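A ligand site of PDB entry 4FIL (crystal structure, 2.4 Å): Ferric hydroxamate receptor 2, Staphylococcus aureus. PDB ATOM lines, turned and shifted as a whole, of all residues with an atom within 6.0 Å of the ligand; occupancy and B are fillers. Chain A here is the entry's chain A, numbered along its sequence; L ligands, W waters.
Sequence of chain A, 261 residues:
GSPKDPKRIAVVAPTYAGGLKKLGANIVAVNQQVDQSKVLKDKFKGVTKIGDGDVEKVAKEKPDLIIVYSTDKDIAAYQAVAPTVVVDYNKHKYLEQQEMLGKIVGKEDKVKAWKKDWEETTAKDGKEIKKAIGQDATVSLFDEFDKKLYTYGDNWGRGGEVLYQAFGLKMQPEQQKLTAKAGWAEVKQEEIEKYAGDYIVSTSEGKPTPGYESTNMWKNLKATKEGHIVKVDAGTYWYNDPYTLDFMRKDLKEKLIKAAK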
ATOM      1  N   PRO A  14      -0.307 -32.730   6.498  1.00  0.00           N
ATOM      2  CA  PRO A  14      -1.717 -32.494   6.122  1.00  0.00           C
ATOM      3  C   PRO A  14      -1.919 -32.012   4.693  1.00  0.00           C
ATOM      4  O   PRO A  14      -3.038 -32.094   4.185  1.00  0.00           O
ATOM      5  CB  PRO A  14      -2.168 -31.401   7.108  1.00  0.00           C
ATOM      6  CG  PRO A  14      -1.082 -31.301   8.135  1.00  0.00           C
ATOM      7  CD  PRO A  14       0.167 -31.780   7.510  1.00  0.00           C
ATOM      8  N   THR A  15      -0.863 -31.527   4.041  1.00  0.00           N
ATOM      9  CA  THR A  15      -0.960 -31.057   2.667  1.00  0.00           C
ATOM     10  C   THR A  15      -1.410 -32.166   1.712  1.00  0.00           C
ATOM     11  O   THR A  15      -2.111 -31.916   0.729  1.00  0.00           O
ATOM     12  CB  THR A  15       0.409 -30.514   2.175  1.00  0.00           C
ATOM     13  OG1 THR A  15       0.875 -29.506   3.083  1.00  0.00           O
ATOM     14  CG2 THR A  15       0.279 -29.913   0.774  1.00  0.00           C
ATOM     15  N   GLN A  33      -5.226 -32.000  11.892  1.00  0.00           N
ATOM     16  CA  GLN A  33      -5.604 -30.695  11.357  1.00  0.00           C
ATOM     17  C   GLN A  33      -6.600 -30.730  10.187  1.00  0.00           C
ATOM     18  O   GLN A  33      -7.100 -29.686   9.779  1.00  0.00           O
ATOM     19  CB  GLN A  33      -4.356 -29.889  11.000  1.00  0.00           C
ATOM     20  CG  GLN A  33      -3.637 -29.332  12.221  1.00  0.00           C
ATOM     21  CD  GLN A  33      -2.256 -28.807  11.903  1.00  0.00           C
ATOM     22  OE1 GLN A  33      -1.589 -29.309  10.995  1.00  0.00           O
ATOM     23  NE2 GLN A  33      -1.810 -27.818  12.663  1.00  0.00           N
ATOM     24  N   TYR A  69       6.670 -33.886   6.211  1.00  0.00           N
ATOM     25  CA  TYR A  69       7.362 -32.736   5.651  1.00  0.00           C
ATOM     26  C   TYR A  69       8.866 -32.897   5.787  1.00  0.00           C
ATOM     27  O   TYR A  69       9.355 -33.671   6.615  1.00  0.00           O
ATOM     28  CB  TYR A  69       6.932 -31.454   6.363  1.00  0.00           C
ATOM     29  CG  TYR A  69       5.500 -31.035   6.091  1.00  0.00           C
ATOM     30  CD1 TYR A  69       5.066 -30.779   4.793  1.00  0.00           C
ATOM     31  CD2 TYR A  69       4.601 -30.861   7.129  1.00  0.00           C
ATOM     32  CE1 TYR A  69       3.765 -30.389   4.542  1.00  0.00           C
ATOM     33  CE2 TYR A  69       3.301 -30.467   6.892  1.00  0.00           C
ATOM     34  CZ  TYR A  69       2.888 -30.233   5.591  1.00  0.00           C
ATOM     35  OH  TYR A  69       1.598 -29.840   5.353  1.00  0.00           O
ATOM     36  N   SER A  70       9.598 -32.185   4.941  1.00  0.00           N
ATOM     37  CA  SER A  70      11.053 -32.210   4.962  1.00  0.00           C
ATOM     38  C   SER A  70      11.641 -31.473   6.179  1.00  0.00           C
ATOM     39  O   SER A  70      12.833 -31.567   6.444  1.00  0.00           O
ATOM     40  CB  SER A  70      11.622 -31.648   3.662  1.00  0.00           C
ATOM     41  OG  SER A  70      11.250 -30.286   3.494  1.00  0.00           O
ATOM     42  N   THR A  71      10.790 -30.749   6.892  1.00  0.00           N
ATOM     43  CA  THR A  71      11.217 -30.042   8.092  1.00  0.00           C
ATOM     44  C   THR A  71      10.725 -30.745   9.352  1.00  0.00           C
ATOM     45  O   THR A  71      10.864 -30.229  10.465  1.00  0.00           O
ATOM     46  CB  THR A  71      10.687 -28.594   8.110  1.00  0.00           C
ATOM     47  OG1 THR A  71       9.261 -28.594   8.212  1.00  0.00           O
ATOM     48  CG2 THR A  71      11.119 -27.855   6.851  1.00  0.00           C
ATOM     49  N   TYR A  89       7.755 -29.402   0.592  1.00  0.00           N
ATOM     50  CA  TYR A  89       6.578 -28.669   0.111  1.00  0.00           C
ATOM     51  C   TYR A  89       6.908 -27.720  -1.044  1.00  0.00           C
ATOM     52  O   TYR A  89       6.176 -27.654  -2.025  1.00  0.00           O
ATOM     53  CB  TYR A  89       5.918 -27.897   1.253  1.00  0.00           C
ATOM     54  CG  TYR A  89       4.713 -27.098   0.801  1.00  0.00           C
ATOM     55  CD1 TYR A  89       3.510 -27.737   0.513  1.00  0.00           C
ATOM     56  CD2 TYR A  89       4.783 -25.725   0.642  1.00  0.00           C
ATOM     57  CE1 TYR A  89       2.407 -27.012   0.081  1.00  0.00           C
ATOM     58  CE2 TYR A  89       3.681 -24.996   0.224  1.00  0.00           C
ATOM     59  CZ  TYR A  89       2.497 -25.648  -0.062  1.00  0.00           C
ATOM     60  OH  TYR A  89       1.405 -24.928  -0.486  1.00  0.00           O
ATOM     61  N   ASN A  90       8.001 -26.976  -0.895  1.00  0.00           N
ATOM     62  CA  ASN A  90       8.395 -25.957  -1.854  1.00  0.00           C
ATOM     63  C   ASN A  90       8.736 -26.491  -3.252  1.00  0.00           C
ATOM     64  O   ASN A  90       8.788 -25.730  -4.218  1.00  0.00           O
ATOM     65  CB  ASN A  90       9.586 -25.169  -1.319  1.00  0.00           C
ATOM     66  CG  ASN A  90       9.209 -24.274  -0.150  1.00  0.00           C
ATOM     67  OD1 ASN A  90       8.073 -23.813  -0.050  1.00  0.00           O
ATOM     68  ND2 ASN A  90      10.165 -24.023   0.742  1.00  0.00           N
ATOM     69  N   ASP A 143      -5.082 -13.091   5.618  1.00  0.00           N
ATOM     70  CA  ASP A 143      -5.331 -14.224   6.503  1.00  0.00           C
ATOM     71  C   ASP A 143      -4.770 -13.966   7.899  1.00  0.00           C
ATOM     72  O   ASP A 143      -3.575 -13.693   8.061  1.00  0.00           O
ATOM     73  CB  ASP A 143      -4.712 -15.490   5.913  1.00  0.00           C
ATOM     74  CG  ASP A 143      -4.868 -16.687   6.823  1.00  0.00           C
ATOM     75  OD1 ASP A 143      -5.970 -16.864   7.400  1.00  0.00           O
ATOM     76  OD2 ASP A 143      -3.895 -17.456   6.975  1.00  0.00           O
ATOM     77  N   GLU A 144      -5.631 -14.050   8.903  1.00  0.00           N
ATOM     78  CA  GLU A 144      -5.221 -13.836  10.286  1.00  0.00           C
ATOM     79  C   GLU A 144      -5.125 -15.140  11.083  1.00  0.00           C
ATOM     80  O   GLU A 144      -6.021 -15.984  11.036  1.00  0.00           O
ATOM     81  CB  GLU A 144      -6.164 -12.855  10.978  1.00  0.00           C
ATOM     82  CG  GLU A 144      -5.869 -12.618  12.451  1.00  0.00           C
ATOM     83  CD  GLU A 144      -6.696 -13.504  13.366  1.00  0.00           C
ATOM     84  OE1 GLU A 144      -7.770 -13.961  12.930  1.00  0.00           O
ATOM     85  OE2 GLU A 144      -6.283 -13.743  14.514  1.00  0.00           O
ATOM     86  N   PHE A 145      -4.030 -15.289  11.819  1.00  0.00           N
ATOM     87  CA  PHE A 145      -3.854 -16.386  12.751  1.00  0.00           C
ATOM     88  C   PHE A 145      -2.971 -15.892  13.890  1.00  0.00           C
ATOM     89  O   PHE A 145      -1.965 -15.213  13.651  1.00  0.00           O
ATOM     90  CB  PHE A 145      -3.203 -17.580  12.050  1.00  0.00           C
ATOM     91  CG  PHE A 145      -3.040 -18.785  12.933  1.00  0.00           C
ATOM     92  CD1 PHE A 145      -1.817 -19.083  13.495  1.00  0.00           C
ATOM     93  CD2 PHE A 145      -4.115 -19.622  13.191  1.00  0.00           C
ATOM     94  CE1 PHE A 145      -1.670 -20.191  14.307  1.00  0.00           C
ATOM     95  CE2 PHE A 145      -3.967 -20.730  14.003  1.00  0.00           C
ATOM     96  CZ  PHE A 145      -2.745 -21.015  14.561  1.00  0.00           C
ATOM     97  N   TYR A 150      -1.395 -12.140   7.555  1.00  0.00           N
ATOM     98  CA  TYR A 150      -0.554 -12.795   6.559  1.00  0.00           C
ATOM     99  C   TYR A 150      -1.106 -12.657   5.133  1.00  0.00           C
ATOM    100  O   TYR A 150      -2.324 -12.611   4.935  1.00  0.00           O
ATOM    101  CB  TYR A 150      -0.410 -14.282   6.903  1.00  0.00           C
ATOM    102  CG  TYR A 150       0.304 -14.540   8.204  1.00  0.00           C
ATOM    103  CD1 TYR A 150       1.685 -14.479   8.302  1.00  0.00           C
ATOM    104  CD2 TYR A 150      -0.416 -14.851   9.357  1.00  0.00           C
ATOM    105  CE1 TYR A 150       2.332 -14.722   9.500  1.00  0.00           C
ATOM    106  CE2 TYR A 150       0.221 -15.095  10.556  1.00  0.00           C
ATOM    107  CZ  TYR A 150       1.589 -15.028  10.624  1.00  0.00           C
ATOM    108  OH  TYR A 150       2.235 -15.266  11.814  1.00  0.00           O
ATOM    109  N   TYR A 152      -0.092 -14.133   0.814  1.00  0.00           N
ATOM    110  CA  TYR A 152       0.505 -15.308   0.186  1.00  0.00           C
ATOM    111  C   TYR A 152       0.739 -15.169  -1.318  1.00  0.00           C
ATOM    112  O   TYR A 152       0.151 -14.305  -1.973  1.00  0.00           O
ATOM    113  CB  TYR A 152      -0.360 -16.540   0.436  1.00  0.00           C
ATOM    114  CG  TYR A 152      -0.667 -16.788   1.895  1.00  0.00           C
ATOM    115  CD1 TYR A 152       0.242 -17.456   2.707  1.00  0.00           C
ATOM    116  CD2 TYR A 152      -1.850 -16.346   2.460  1.00  0.00           C
ATOM    117  CE1 TYR A 152      -0.024 -17.671   4.044  1.00  0.00           C
ATOM    118  CE2 TYR A 152      -2.126 -16.561   3.797  1.00  0.00           C
ATOM    119  CZ  TYR A 152      -1.218 -17.228   4.587  1.00  0.00           C
ATOM    120  OH  TYR A 152      -1.494 -17.438   5.916  1.00  0.00           O
ATOM    121  N   ASN A 155       0.825 -20.254  -4.428  1.00  0.00           N
ATOM    122  CA  ASN A 155       0.852 -21.658  -4.040  1.00  0.00           C
ATOM    123  C   ASN A 155       1.099 -21.901  -2.548  1.00  0.00           C
ATOM    124  O   ASN A 155       1.947 -22.707  -2.179  1.00  0.00           O
ATOM    125  CB  ASN A 155       1.885 -22.434  -4.876  1.00  0.00           C
ATOM    126  CG  ASN A 155       1.511 -23.892  -5.055  1.00  0.00           C
ATOM    127  OD1 ASN A 155       1.123 -24.315  -6.131  1.00  0.00           O
ATOM    128  ND2 ASN A 155       1.637 -24.664  -3.981  1.00  0.00           N
ATOM    129  N   TRP A 156       0.358 -21.189  -1.700  1.00  0.00           N
ATOM    130  CA  TRP A 156       0.460 -21.384  -0.263  1.00  0.00           C
ATOM    131  C   TRP A 156      -0.907 -21.484   0.399  1.00  0.00           C
ATOM    132  O   TRP A 156      -1.107 -20.994   1.521  1.00  0.00           O
ATOM    133  CB  TRP A 156       1.268 -20.251   0.380  1.00  0.00           C
ATOM    134  CG  TRP A 156       2.084 -20.701   1.565  1.00  0.00           C
ATOM    135  CD1 TRP A 156       1.706 -20.676   2.872  1.00  0.00           C
ATOM    136  CD2 TRP A 156       3.405 -21.250   1.528  1.00  0.00           C
ATOM    137  NE1 TRP A 156       2.725 -21.164   3.664  1.00  0.00           N
ATOM    138  CE2 TRP A 156       3.770 -21.526   2.866  1.00  0.00           C
ATOM    139  CE3 TRP A 156       4.314 -21.529   0.510  1.00  0.00           C
ATOM    140  CZ2 TRP A 156       5.007 -22.072   3.194  1.00  0.00           C
ATOM    141  CZ3 TRP A 156       5.541 -22.075   0.839  1.00  0.00           C
ATOM    142  CH2 TRP A 156       5.876 -22.337   2.176  1.00  0.00           C
ATOM    143  N   GLY A 157      -1.848 -22.117  -0.284  1.00  0.00           N
ATOM    144  CA  GLY A 157      -3.205 -22.258   0.227  1.00  0.00           C
ATOM    145  C   GLY A 157      -3.993 -20.970   0.138  1.00  0.00           C
ATOM    146  O   GLY A 157      -3.603 -20.056  -0.592  1.00  0.00           O
ATOM    147  N   ARG A 158      -5.104 -20.917   0.858  1.00  0.00           N
ATOM    148  CA  ARG A 158      -5.929 -19.709   0.956  1.00  0.00           C
ATOM    149  C   ARG A 158      -6.594 -19.317  -0.363  1.00  0.00           C
ATOM    150  O   ARG A 158      -7.037 -18.177  -0.538  1.00  0.00           O
ATOM    151  CB  ARG A 158      -5.152 -18.540   1.576  1.00  0.00           C
ATOM    152  CG  ARG A 158      -4.815 -18.707   3.070  1.00  0.00           C
ATOM    153  CD  ARG A 158      -3.647 -19.664   3.297  1.00  0.00           C
ATOM    154  NE  ARG A 158      -3.305 -19.801   4.715  1.00  0.00           N
ATOM    155  CZ  ARG A 158      -2.330 -20.572   5.176  1.00  0.00           C
ATOM    156  NH1 ARG A 158      -1.599 -21.284   4.329  1.00  0.00           N
ATOM    157  NH2 ARG A 158      -2.087 -20.640   6.480  1.00  0.00           N
ATOM    158  N   TRP A 184       4.958 -16.650   1.205  1.00  0.00           N
ATOM    159  CA  TRP A 184       4.111 -16.096   2.259  1.00  0.00           C
ATOM    160  C   TRP A 184       4.863 -14.980   2.954  1.00  0.00           C
ATOM    161  O   TRP A 184       6.086 -14.861   2.819  1.00  0.00           O
ATOM    162  CB  TRP A 184       3.751 -17.181   3.270  1.00  0.00           C
ATOM    163  CG  TRP A 184       4.920 -17.683   4.055  1.00  0.00           C
ATOM    164  CD1 TRP A 184       5.795 -18.671   3.686  1.00  0.00           C
ATOM    165  CD2 TRP A 184       5.362 -17.217   5.336  1.00  0.00           C
ATOM    166  NE1 TRP A 184       6.747 -18.850   4.668  1.00  0.00           N
ATOM    167  CE2 TRP A 184       6.499 -17.965   5.683  1.00  0.00           C
ATOM    168  CE3 TRP A 184       4.904 -16.235   6.213  1.00  0.00           C
ATOM    169  CZ2 TRP A 184       7.186 -17.769   6.874  1.00  0.00           C
ATOM    170  CZ3 TRP A 184       5.580 -16.039   7.405  1.00  0.00           C
ATOM    171  CH2 TRP A 184       6.715 -16.803   7.721  1.00  0.00           C
ATOM    172  N   ALA A 185       4.136 -14.165   3.721  1.00  0.00           N
ATOM    173  CA  ALA A 185       4.730 -13.050   4.450  1.00  0.00           C
ATOM    174  C   ALA A 185       3.737 -12.446   5.428  1.00  0.00           C
ATOM    175  O   ALA A 185       2.534 -12.400   5.148  1.00  0.00           O
ATOM    176  CB  ALA A 185       5.232 -11.994   3.481  1.00  0.00           C
ATOM    177  N   TRP A 238      -6.999 -23.664   4.111  1.00  0.00           N
ATOM    178  CA  TRP A 238      -5.590 -23.941   4.337  1.00  0.00           C
ATOM    179  C   TRP A 238      -5.036 -24.855   3.250  1.00  0.00           C
ATOM    180  O   TRP A 238      -3.843 -24.845   2.963  1.00  0.00           O
ATOM    181  CB  TRP A 238      -5.373 -24.611   5.692  1.00  0.00           C
ATOM    182  CG  TRP A 238      -5.590 -23.717   6.872  1.00  0.00           C
ATOM    183  CD1 TRP A 238      -5.659 -22.355   6.866  1.00  0.00           C
ATOM    184  CD2 TRP A 238      -5.764 -24.122   8.232  1.00  0.00           C
ATOM    185  NE1 TRP A 238      -5.869 -21.882   8.140  1.00  0.00           N
ATOM    186  CE2 TRP A 238      -5.929 -22.951   9.000  1.00  0.00           C
ATOM    187  CE3 TRP A 238      -5.788 -25.359   8.880  1.00  0.00           C
ATOM    188  CZ2 TRP A 238      -6.131 -22.985  10.378  1.00  0.00           C
ATOM    189  CZ3 TRP A 238      -5.981 -25.388  10.248  1.00  0.00           C
ATOM    190  CH2 TRP A 238      -6.149 -24.212  10.985  1.00  0.00           C
ATOM    191  N   TYR A 239      -5.932 -25.635   2.640  1.00  0.00           N
ATOM    192  CA  TYR A 239      -5.523 -26.753   1.781  1.00  0.00           C
ATOM    193  C   TYR A 239      -5.529 -26.461   0.288  1.00  0.00           C
ATOM    194  O   TYR A 239      -6.081 -25.451  -0.159  1.00  0.00           O
ATOM    195  CB  TYR A 239      -6.394 -27.969   2.086  1.00  0.00           C
ATOM    196  CG  TYR A 239      -6.243 -28.485   3.499  1.00  0.00           C
ATOM    197  CD1 TYR A 239      -7.001 -27.962   4.540  1.00  0.00           C
ATOM    198  CD2 TYR A 239      -5.330 -29.485   3.800  1.00  0.00           C
ATOM    199  CE1 TYR A 239      -6.859 -28.432   5.830  1.00  0.00           C
ATOM    200  CE2 TYR A 239      -5.178 -29.955   5.089  1.00  0.00           C
ATOM    201  CZ  TYR A 239      -5.948 -29.426   6.100  1.00  0.00           C
ATOM    202  OH  TYR A 239      -5.796 -29.896   7.390  1.00  0.00           O
ATOM    203  N   ASN A 240      -4.911 -27.356  -0.471  1.00  0.00           N
ATOM    204  CA  ASN A 240      -4.865 -27.259  -1.928  1.00  0.00           C
ATOM    205  C   ASN A 240      -5.022 -28.640  -2.585  1.00  0.00           C
ATOM    206  O   ASN A 240      -4.467 -28.897  -3.657  1.00  0.00           O
ATOM    207  CB  ASN A 240      -3.574 -26.583  -2.385  1.00  0.00           C
ATOM    208  CG  ASN A 240      -2.328 -27.215  -1.783  1.00  0.00           C
ATOM    209  OD1 ASN A 240      -2.378 -28.314  -1.217  1.00  0.00           O
ATOM    210  ND2 ASN A 240      -1.202 -26.516  -1.881  1.00  0.00           N
HETATM  211 FE1  LIG L   1       1.286 -23.304   6.987  1.00  0.00          FE
HETATM  212  O1  LIG L   1       2.629 -24.373   5.997  1.00  0.00           O
HETATM  213  O2  LIG L   1       0.481 -23.361   5.111  1.00  0.00           O
HETATM  214  O3  LIG L   1       0.392 -24.920   7.677  1.00  0.00           O
HETATM  215  O4  LIG L   1      -0.423 -22.521   7.760  1.00  0.00           O
HETATM  216  O5  LIG L   1       1.958 -21.449   6.828  1.00  0.00           O
HETATM  217  O6  LIG L   1       2.504 -23.199   8.607  1.00  0.00           O
HETATM  218  N1  LIG L   1       2.217 -24.719   4.724  1.00  0.00           N
HETATM  219  C1  LIG L   1       1.094 -24.168   4.298  1.00  0.00           C
HETATM  220  C2  LIG L   1       0.457 -24.375   2.959  1.00  0.00           C
HETATM  221  C3  LIG L   1       0.254 -25.819   2.500  1.00  0.00           C
HETATM  222  C4  LIG L   1      -1.108 -26.434   2.812  1.00  0.00           C
HETATM  223  O7  LIG L   1      -1.945 -26.563   1.900  1.00  0.00           O
HETATM  224  N2  LIG L   1      -1.281 -26.814   4.048  1.00  0.00           N
HETATM  225  C5  LIG L   1      -2.511 -27.429   4.513  1.00  0.00           C
HETATM  226  C6  LIG L   1      -2.407 -27.836   5.980  1.00  0.00           C
HETATM  227  C7  LIG L   1      -1.478 -26.984   8.171  1.00  0.00           C
HETATM  228  C8  LIG L   1      -2.269 -26.662   6.924  1.00  0.00           C
HETATM  229  C9  LIG L   1      -1.281 -25.792   9.098  1.00  0.00           C
HETATM  230  N3  LIG L   1      -0.717 -24.632   8.426  1.00  0.00           N
HETATM  231  C10 LIG L   1      -1.096 -23.373   8.442  1.00  0.00           C
HETATM  232  C11 LIG L   1      -2.284 -22.902   9.219  1.00  0.00           C
HETATM  233  C12 LIG L   1      -1.912 -21.949  10.355  1.00  0.00           C
HETATM  234  C13 LIG L   1      -1.666 -20.532   9.863  1.00  0.00           C
HETATM  235  O8  LIG L   1      -2.487 -19.956   9.165  1.00  0.00           O
HETATM  236  N4  LIG L   1      -0.506 -19.974  10.236  1.00  0.00           N
HETATM  237  C14 LIG L   1      -0.111 -18.626   9.855  1.00  0.00           C
HETATM  238  C15 LIG L   1       1.189 -18.549   9.115  1.00  0.00           C
HETATM  239  C16 LIG L   1       1.161 -18.529   7.596  1.00  0.00           C
HETATM  240  C17 LIG L   1       2.482 -18.773   6.996  1.00  0.00           C
HETATM  241  C18 LIG L   1       3.400 -19.762   7.786  1.00  0.00           C
HETATM  242  N5  LIG L   1       2.841 -21.118   7.828  1.00  0.00           N
HETATM  243  C19 LIG L   1       3.085 -22.070   8.723  1.00  0.00           C
HETATM  244  C20 LIG L   1       4.038 -21.841   9.856  1.00  0.00           C
HETATM  245  C21 LIG L   1       3.165 -25.649   4.106  1.00  0.00           C
HETATM  246  C22 LIG L   1       3.606 -26.709   5.098  1.00  0.00           C
HETATM  247  C23 LIG L   1       5.095 -27.088   5.030  1.00  0.00           C
HETATM  248  C24 LIG L   1       5.763 -27.214   6.386  1.00  0.00           C
HETATM  249  C25 LIG L   1       7.268 -27.116   6.266  1.00  0.00           C
HETATM  250  N6  LIG L   1       7.711 -25.762   5.851  1.00  0.00           N
HETATM  251  O   HOH W   1       8.971 -28.607   3.859  1.00  0.00           O
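O8 of the ligand lies within hydrogen-bond range of NH2 of Arg 158 (2.8 Å).
The backbone carbonyl oxygen of Trp 238 sits close to a nitrogen (N2) of the ligand (3.4 Å).
The guanidinium group (NH1) of Arg 158 sits at hydrogen-bond distance from the backbone carbonyl oxygen (O) of Trp 156 (2.9 Å).
OH of Tyr 89 is in hydrogen-bond range of O of Asn 155 (2.8 Å).
The side-chain hydroxyl of Tyr 239 sits at hydrogen-bond distance from the backbone carbonyl oxygen of Gln 33.
The side-chain carboxylate of Asp 143 is in salt-bridge range of the guanidinium group of Arg 158, 3.3 Å away.
The side-chain carboxylate of Asp 143 is in hydrogen-bond range of the side-chain hydroxyl of Tyr 152 (2.6 Å).
The backbone NH (N) of Tyr 150 lies within hydrogen-bond range of the backbone carbonyl oxygen (O) of Asp 143, at 2.7 Å.
The side-chain hydroxyl of Tyr 152 is in hydrogen-bond range of the guanidinium group of Arg 158, 3.2 Å away.
The side-chain hydroxyl of Tyr 69 is in hydrogen-bond range of the side-chain hydroxyl of Thr 15, 2.4 Å away.
NE1 of Trp 156 sits close to O5 of the ligand (3.3 Å).
CB of Pro 14 touches C6 of the ligand (3.7 Å).
OG1 of Thr 15 touches N2 of the ligand (3.6 Å).
Gln 33 touches the ligand (OE1 to C7, 3.7 Å).
CE1 of Tyr 69 touches C23 of the ligand (3.6 Å).
Thr 71 touches the ligand (OG1 to C25, 3.2 Å).
Tyr 89 touches the ligand (OH to C3, 3.3 Å).
Asp 143 touches the ligand (OD2 to O8, 3.6 Å).
Phe 145 touches the ligand.
CE2 of Tyr 150 touches C14 of the ligand, 3.6 Å away.
OH of Tyr 152 touches C16 of the ligand, 3.3 Å away.
Trp 184 touches the ligand.
Tyr 239 touches the ligand.
Asn 240 touches the ligand.
Hydrophobic or aromatic side chains within 4 Å of the ligand: Pro 14, Tyr 69, Tyr 89, Phe 145, Tyr 150, Tyr 152, Trp 156, Trp 184, Trp 238 and Tyr 239.
Along chain A the residues within 4 Å of the ligand span positions 14 to 240.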
